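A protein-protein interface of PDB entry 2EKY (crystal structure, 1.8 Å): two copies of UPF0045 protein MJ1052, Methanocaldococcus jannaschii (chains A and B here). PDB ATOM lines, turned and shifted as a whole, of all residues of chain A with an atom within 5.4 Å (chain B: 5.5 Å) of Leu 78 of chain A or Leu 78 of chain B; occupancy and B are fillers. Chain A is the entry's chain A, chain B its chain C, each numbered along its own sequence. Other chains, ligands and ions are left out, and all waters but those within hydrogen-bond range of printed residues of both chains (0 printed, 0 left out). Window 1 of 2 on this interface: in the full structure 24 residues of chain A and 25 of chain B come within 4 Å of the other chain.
The backbone NH of Lys 79 of chain A lies within hydrogen-bond range of the backbone carbonyl oxygen of Glu 10 of chain A, at 2.9 Å.
O of Ser 12 of chain A lies within hydrogen-bond range of N of Ser 77 of chain A.
O of Glu 10 of chain B is in hydrogen-bond range of N of Lys 79 of chain B (2.9 Å).
The backbone carbonyl oxygen (O) of Ser 12 of chain B is in hydrogen-bond range of the backbone NH (N) of Ser 77 of chain B (2.8 Å).
Of the 12 printed residues of chain B, 5 touch a printed residue of chain A.
Hydrophobic or aromatic side chains of chain B that line the printed part of chain A: Leu 78 and Ile 80.
Among the printed residues, no Asp or Glu carboxylate lies within 4 Å of a Lys or Arg side-chain nitrogen of the other chain.
The backbone carbonyl oxygen (O) of Ser 76 of chain A is in hydrogen-bond range of the backbone NH (N) of Ile 80 of chain B.
The backbone NH of Leu 78 of chain A is in hydrogen-bond range of the backbone carbonyl oxygen of Leu 78 of chain B (2.7 Å).
The backbone NH (N) of Ile 80 of chain A sits at hydrogen-bond distance from the backbone carbonyl oxygen (O) of Ser 76 of chain B.
Ser 76 of chain A touches Lys 79 of chain B, and with the chains exchanged Lys 79 of chain A touches Ser 76 of chain B.
Ser 76 of chain A touches Ile 80 of chain B, and with the chains exchanged Ile 80 of chain A touches Ser 76 of chain B.
Ser 77 of chain A touches Leu 78 of chain B, and with the chains exchanged Leu 78 of chain A touches Ser 77 of chain B.
Ser 77 of chain A touches Lys 79 of chain B, and with the chains exchanged Lys 79 of chain A touches Ser 77 of chain B.
12 positions are printed for both chains.
Of the 11 pairs that touch across the chains among the printed residues, 11 have their exchanged pair printed and touching as well.
Leu 78 of chain B touches Ser 76 of chain A (O to O, 3.9 Å).
Ser 76 of chain A touches Lys 79 of chain B.
O of Leu 78 of chain B touches CA of Ser 77 of chain A, 3.3 Å away.
CE of Lys 79 of chain B touches OG of Ser 77 of chain A, at 3.7 Å.
Leu 78 of chain A touches Ser 76 of chain B (O to O, 3.8 Å).
O of Leu 78 of chain A touches CA of Ser 77 of chain B, at 3.3 Å.
O of Ser 76 of chain B touches CA of Lys 79 of chain A, 3.2 Å away.
OG of Ser 77 of chain B touches CE of Lys 79 of chain A, at 3.7 Å.
Leu 78 of chain A touches just these residues of chain B: Ser 76 (3.8 Å), Ser 77 (3.3 Å) and Leu 78 (2.7 Å).
Leu 78 of chain B touches three residues of chain A.
Printed residues of chain B within 4 Å of Lys 79 of chain A: Ser 76 and Ser 77.
Of the printed residues of chain B, Ile 80 of chain A touches Ser 76.
Printed residues of chain A within 4 Å of Lys 79 of chain B: Ser 76 and Ser 77.
Phe 60 of chain A touches none of the printed residues of chain B.
Glu 10 of chain A touches none of the printed residues of chain B.
The nearest residue of chain A that does not touch Leu 78 of chain B is Phe 60 of chain A (4.2 Å).
The nearest printed residue of chain B that does not touch Ser 77 of chain A is Ile 80 of chain B (4.9 Å).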
ATOM      1  N   ALA A   9      10.747 -14.963  13.896  1.00  0.00           N
ATOM      2  CA  ALA A   9      12.106 -14.538  14.184  1.00  0.00           C
ATOM      3  C   ALA A   9      12.776 -15.373  15.254  1.00  0.00           C
ATOM      4  O   ALA A   9      12.131 -16.158  15.942  1.00  0.00           O
ATOM      5  CB  ALA A   9      12.098 -13.080  14.628  1.00  0.00           C
ATOM      6  N   GLU A  10      14.086 -15.203  15.376  1.00  0.00           N
ATOM      7  CA  GLU A  10      14.826 -15.898  16.414  1.00  0.00           C
ATOM      8  C   GLU A  10      15.738 -14.891  17.092  1.00  0.00           C
ATOM      9  O   GLU A  10      16.368 -14.059  16.434  1.00  0.00           O
ATOM     10  CB  GLU A  10      15.646 -17.051  15.848  1.00  0.00           C
ATOM     11  CG  GLU A  10      16.363 -17.851  16.942  1.00  0.00           C
ATOM     12  CD  GLU A  10      16.970 -19.134  16.424  1.00  0.00           C
ATOM     13  OE1 GLU A  10      17.699 -19.068  15.412  1.00  0.00           O
ATOM     14  OE2 GLU A  10      16.712 -20.203  17.027  1.00  0.00           O
ATOM     15  N   VAL A  11      15.787 -14.967  18.416  1.00  0.00           N
ATOM     16  CA  VAL A  11      16.612 -14.081  19.217  1.00  0.00           C
ATOM     17  C   VAL A  11      17.544 -14.900  20.102  1.00  0.00           C
ATOM     18  O   VAL A  11      17.118 -15.865  20.734  1.00  0.00           O
ATOM     19  CB  VAL A  11      15.742 -13.187  20.140  1.00  0.00           C
ATOM     20  CG1 VAL A  11      16.632 -12.372  21.067  1.00  0.00           C
ATOM     21  CG2 VAL A  11      14.871 -12.256  19.297  1.00  0.00           C
ATOM     22  N   SER A  12      18.815 -14.520  20.127  1.00  0.00           N
ATOM     23  CA  SER A  12      19.784 -15.187  20.983  1.00  0.00           C
ATOM     24  C   SER A  12      20.518 -14.061  21.685  1.00  0.00           C
ATOM     25  O   SER A  12      20.935 -13.088  21.056  1.00  0.00           O
ATOM     26  CB  SER A  12      20.761 -16.051  20.174  1.00  0.00           C
ATOM     27  OG  SER A  12      21.701 -15.266  19.472  1.00  0.00           O
ATOM     28  N   ILE A  56       8.282  -7.143  17.661  1.00  0.00           N
ATOM     29  CA  ILE A  56       9.468  -7.974  17.833  1.00  0.00           C
ATOM     30  C   ILE A  56      10.703  -7.099  18.009  1.00  0.00           C
ATOM     31  O   ILE A  56      11.558  -7.384  18.851  1.00  0.00           O
ATOM     32  CB  ILE A  56       9.645  -8.928  16.631  1.00  0.00           C
ATOM     33  CG1 ILE A  56       8.573 -10.019  16.702  1.00  0.00           C
ATOM     34  CG2 ILE A  56      11.054  -9.525  16.624  1.00  0.00           C
ATOM     35  CD1 ILE A  56       8.574 -10.994  15.545  1.00  0.00           C
ATOM     36  N   LEU A  57      10.791  -6.025  17.230  1.00  0.00           N
ATOM     37  CA  LEU A  57      11.930  -5.120  17.331  1.00  0.00           C
ATOM     38  C   LEU A  57      11.972  -4.450  18.705  1.00  0.00           C
ATOM     39  O   LEU A  57      13.046  -4.272  19.279  1.00  0.00           O
ATOM     40  CB  LEU A  57      11.869  -4.070  16.217  1.00  0.00           C
ATOM     41  CG  LEU A  57      12.188  -4.634  14.824  1.00  0.00           C
ATOM     42  CD1 LEU A  57      11.797  -3.634  13.751  1.00  0.00           C
ATOM     43  CD2 LEU A  57      13.672  -4.970  14.739  1.00  0.00           C
ATOM     44  N   PHE A  60      12.853  -7.143  21.300  1.00  0.00           N
ATOM     45  CA  PHE A  60      14.274  -7.449  21.163  1.00  0.00           C
ATOM     46  C   PHE A  60      15.095  -6.404  21.909  1.00  0.00           C
ATOM     47  O   PHE A  60      15.970  -6.738  22.710  1.00  0.00           O
ATOM     48  CB  PHE A  60      14.666  -7.457  19.682  1.00  0.00           C
ATOM     49  CG  PHE A  60      16.142  -7.645  19.436  1.00  0.00           C
ATOM     50  CD1 PHE A  60      16.782  -8.824  19.806  1.00  0.00           C
ATOM     51  CD2 PHE A  60      16.890  -6.638  18.831  1.00  0.00           C
ATOM     52  CE1 PHE A  60      18.147  -8.997  19.575  1.00  0.00           C
ATOM     53  CE2 PHE A  60      18.256  -6.798  18.592  1.00  0.00           C
ATOM     54  CZ  PHE A  60      18.887  -7.981  18.967  1.00  0.00           C
ATOM     55  N   SER A  76      23.656  -9.502  21.375  1.00  0.00           N
ATOM     56  CA  SER A  76      22.342 -10.038  21.037  1.00  0.00           C
ATOM     57  C   SER A  76      22.101 -10.085  19.537  1.00  0.00           C
ATOM     58  O   SER A  76      22.477  -9.168  18.806  1.00  0.00           O
ATOM     59  CB  SER A  76      21.250  -9.199  21.700  1.00  0.00           C
ATOM     60  OG  SER A  76      21.444  -9.129  23.106  1.00  0.00           O
ATOM     61  N   SER A  77      21.453 -11.157  19.092  1.00  0.00           N
ATOM     62  CA  SER A  77      21.167 -11.359  17.677  1.00  0.00           C
ATOM     63  C   SER A  77      19.673 -11.488  17.410  1.00  0.00           C
ATOM     64  O   SER A  77      18.942 -12.088  18.190  1.00  0.00           O
ATOM     65  CB  SER A  77      21.866 -12.631  17.176  1.00  0.00           C
ATOM     66  OG  SER A  77      23.248 -12.598  17.474  1.00  0.00           O
ATOM     67  N   LEU A  78      19.234 -10.922  16.293  1.00  0.00           N
ATOM     68  CA  LEU A  78      17.839 -10.991  15.898  1.00  0.00           C
ATOM     69  C   LEU A  78      17.813 -11.389  14.428  1.00  0.00           C
ATOM     70  O   LEU A  78      18.442 -10.739  13.592  1.00  0.00           O
ATOM     71  CB  LEU A  78      17.152  -9.628  16.079  1.00  0.00           C
ATOM     72  CG  LEU A  78      15.741  -9.498  15.485  1.00  0.00           C
ATOM     73  CD1 LEU A  78      14.774 -10.423  16.212  1.00  0.00           C
ATOM     74  CD2 LEU A  78      15.270  -8.042  15.584  1.00  0.00           C
ATOM     75  N   LYS A  79      17.113 -12.474  14.128  1.00  0.00           N
ATOM     76  CA  LYS A  79      16.990 -12.941  12.758  1.00  0.00           C
ATOM     77  C   LYS A  79      15.510 -12.911  12.414  1.00  0.00           C
ATOM     78  O   LYS A  79      14.673 -13.389  13.184  1.00  0.00           O
ATOM     79  CB  LYS A  79      17.548 -14.361  12.621  1.00  0.00           C
ATOM     80  CG  LYS A  79      17.476 -14.909  11.203  1.00  0.00           C
ATOM     81  CD  LYS A  79      18.039 -16.321  11.107  1.00  0.00           C
ATOM     82  CE  LYS A  79      19.541 -16.356  11.356  1.00  0.00           C
ATOM     83  NZ  LYS A  79      20.075 -17.752  11.268  1.00  0.00           N
ATOM     84  N   ILE A  80      15.192 -12.340  11.257  1.00  0.00           N
ATOM     85  CA  ILE A  80      13.810 -12.219  10.813  1.00  0.00           C
ATOM     86  C   ILE A  80      13.583 -12.966   9.504  1.00  0.00           C
ATOM     87  O   ILE A  80      14.379 -12.858   8.580  1.00  0.00           O
ATOM     88  CB  ILE A  80      13.429 -10.736  10.541  1.00  0.00           C
ATOM     89  CG1 ILE A  80      13.726  -9.856  11.765  1.00  0.00           C
ATOM     90  CG2 ILE A  80      11.956 -10.647  10.141  1.00  0.00           C
ATOM     91  CD1 ILE A  80      12.884 -10.144  12.979  1.00  0.00           C
ATOM     92  N   ALA B   9      27.159  -2.814  15.441  1.00  0.00           N
ATOM     93  CA  ALA B   9      26.314  -3.907  14.991  1.00  0.00           C
ATOM     94  C   ALA B   9      26.717  -4.430  13.635  1.00  0.00           C
ATOM     95  O   ALA B   9      27.569  -3.854  12.964  1.00  0.00           O
ATOM     96  CB  ALA B   9      24.863  -3.439  14.947  1.00  0.00           C
ATOM     97  N   GLU B  10      26.103  -5.545  13.248  1.00  0.00           N
ATOM     98  CA  GLU B  10      26.344  -6.135  11.944  1.00  0.00           C
ATOM     99  C   GLU B  10      25.018  -6.614  11.367  1.00  0.00           C
ATOM    100  O   GLU B  10      24.220  -7.271  12.044  1.00  0.00           O
ATOM    101  CB  GLU B  10      27.331  -7.300  12.024  1.00  0.00           C
ATOM    102  CG  GLU B  10      27.692  -7.849  10.644  1.00  0.00           C
ATOM    103  CD  GLU B  10      28.840  -8.829  10.676  1.00  0.00           C
ATOM    104  OE1 GLU B  10      28.793  -9.768  11.494  1.00  0.00           O
ATOM    105  OE2 GLU B  10      29.791  -8.662   9.877  1.00  0.00           O
ATOM    106  N   VAL B  11      24.792  -6.277  10.106  1.00  0.00           N
ATOM    107  CA  VAL B  11      23.565  -6.650   9.424  1.00  0.00           C
ATOM    108  C   VAL B  11      23.845  -7.474   8.174  1.00  0.00           C
ATOM    109  O   VAL B  11      24.807  -7.217   7.457  1.00  0.00           O
ATOM    110  CB  VAL B  11      22.774  -5.382   8.997  1.00  0.00           C
ATOM    111  CG1 VAL B  11      21.587  -5.768   8.127  1.00  0.00           C
ATOM    112  CG2 VAL B  11      22.306  -4.624  10.228  1.00  0.00           C
ATOM    113  N   SER B  12      23.004  -8.472   7.930  1.00  0.00           N
ATOM    114  CA  SER B  12      23.107  -9.294   6.734  1.00  0.00           C
ATOM    115  C   SER B  12      21.674  -9.483   6.252  1.00  0.00           C
ATOM    116  O   SER B  12      20.787  -9.846   7.029  1.00  0.00           O
ATOM    117  CB  SER B  12      23.740 -10.658   7.029  1.00  0.00           C
ATOM    118  OG  SER B  12      22.836 -11.506   7.712  1.00  0.00           O
ATOM    119  N   ILE B  56      19.859   2.247  14.524  1.00  0.00           N
ATOM    120  CA  ILE B  56      20.263   1.009  13.865  1.00  0.00           C
ATOM    121  C   ILE B  56      19.043   0.090  13.706  1.00  0.00           C
ATOM    122  O   ILE B  56      18.883  -0.575  12.678  1.00  0.00           O
ATOM    123  CB  ILE B  56      21.403   0.317  14.664  1.00  0.00           C
ATOM    124  CG1 ILE B  56      22.715   1.070  14.408  1.00  0.00           C
ATOM    125  CG2 ILE B  56      21.534  -1.154  14.271  1.00  0.00           C
ATOM    126  CD1 ILE B  56      23.923   0.509  15.122  1.00  0.00           C
ATOM    127  N   LEU B  57      18.175   0.065  14.713  1.00  0.00           N
ATOM    128  CA  LEU B  57      16.971  -0.759  14.641  1.00  0.00           C
ATOM    129  C   LEU B  57      16.073  -0.287  13.492  1.00  0.00           C
ATOM    130  O   LEU B  57      15.487  -1.097  12.768  1.00  0.00           O
ATOM    131  CB  LEU B  57      16.210  -0.694  15.967  1.00  0.00           C
ATOM    132  CG  LEU B  57      16.881  -1.453  17.120  1.00  0.00           C
ATOM    133  CD1 LEU B  57      16.183  -1.143  18.433  1.00  0.00           C
ATOM    134  CD2 LEU B  57      16.843  -2.948  16.830  1.00  0.00           C
ATOM    135  N   PHE B  60      17.810  -1.021  10.116  1.00  0.00           N
ATOM    136  CA  PHE B  60      17.726  -2.463   9.873  1.00  0.00           C
ATOM    137  C   PHE B  60      16.359  -2.798   9.281  1.00  0.00           C
ATOM    138  O   PHE B  60      16.259  -3.458   8.242  1.00  0.00           O
ATOM    139  CB  PHE B  60      17.928  -3.231  11.184  1.00  0.00           C
ATOM    140  CG  PHE B  60      17.676  -4.715  11.071  1.00  0.00           C
ATOM    141  CD1 PHE B  60      18.496  -5.522  10.287  1.00  0.00           C
ATOM    142  CD2 PHE B  60      16.616  -5.299  11.749  1.00  0.00           C
ATOM    143  CE1 PHE B  60      18.259  -6.898  10.181  1.00  0.00           C
ATOM    144  CE2 PHE B  60      16.365  -6.671  11.653  1.00  0.00           C
ATOM    145  CZ  PHE B  60      17.189  -7.471  10.869  1.00  0.00           C
ATOM    146  N   SER B  76      16.715 -11.704   7.263  1.00  0.00           N
ATOM    147  CA  SER B  76      17.640 -10.667   7.695  1.00  0.00           C
ATOM    148  C   SER B  76      18.124 -10.876   9.118  1.00  0.00           C
ATOM    149  O   SER B  76      17.380 -11.342   9.977  1.00  0.00           O
ATOM    150  CB  SER B  76      16.968  -9.298   7.577  1.00  0.00           C
ATOM    151  OG  SER B  76      16.562  -9.067   6.239  1.00  0.00           O
ATOM    152  N   SER B  77      19.380 -10.517   9.357  1.00  0.00           N
ATOM    153  CA  SER B  77      19.977 -10.678  10.674  1.00  0.00           C
ATOM    154  C   SER B  77      20.604  -9.395  11.175  1.00  0.00           C
ATOM    155  O   SER B  77      21.251  -8.666  10.421  1.00  0.00           O
ATOM    156  CB  SER B  77      21.061 -11.760  10.645  1.00  0.00           C
ATOM    157  OG  SER B  77      20.522 -13.008  10.262  1.00  0.00           O
ATOM    158  N   LEU B  78      20.414  -9.152  12.464  1.00  0.00           N
ATOM    159  CA  LEU B  78      20.963  -7.990  13.138  1.00  0.00           C
ATOM    160  C   LEU B  78      21.659  -8.475  14.402  1.00  0.00           C
ATOM    161  O   LEU B  78      21.052  -9.166  15.220  1.00  0.00           O
ATOM    162  CB  LEU B  78      19.849  -7.024  13.534  1.00  0.00           C
ATOM    163  CG  LEU B  78      20.294  -5.874  14.441  1.00  0.00           C
ATOM    164  CD1 LEU B  78      21.297  -5.013  13.701  1.00  0.00           C
ATOM    165  CD2 LEU B  78      19.080  -5.047  14.867  1.00  0.00           C
ATOM    166  N   LYS B  79      22.932  -8.129  14.555  1.00  0.00           N
ATOM    167  CA  LYS B  79      23.677  -8.511  15.747  1.00  0.00           C
ATOM    168  C   LYS B  79      24.144  -7.224  16.414  1.00  0.00           C
ATOM    169  O   LYS B  79      24.725  -6.354  15.760  1.00  0.00           O
ATOM    170  CB  LYS B  79      24.880  -9.380  15.377  1.00  0.00           C
ATOM    171  CG  LYS B  79      25.705  -9.819  16.573  1.00  0.00           C
ATOM    172  CD  LYS B  79      26.853 -10.725  16.143  1.00  0.00           C
ATOM    173  CE  LYS B  79      26.348 -12.007  15.505  1.00  0.00           C
ATOM    174  NZ  LYS B  79      27.455 -12.743  14.821  1.00  0.00           N
ATOM    175  N   ILE B  80      23.880  -7.105  17.711  1.00  0.00           N
ATOM    176  CA  ILE B  80      24.253  -5.918  18.476  1.00  0.00           C
ATOM    177  C   ILE B  80      25.304  -6.257  19.523  1.00  0.00           C
ATOM    178  O   ILE B  80      25.178  -7.251  20.229  1.00  0.00           O
ATOM    179  CB  ILE B  80      23.024  -5.328  19.213  1.00  0.00           C
ATOM    180  CG1 ILE B  80      21.914  -5.010  18.207  1.00  0.00           C
ATOM    181  CG2 ILE B  80      23.427  -4.093  20.015  1.00  0.00           C
ATOM    182  CD1 ILE B  80      22.328  -4.072  17.112  1.00  0.00           C
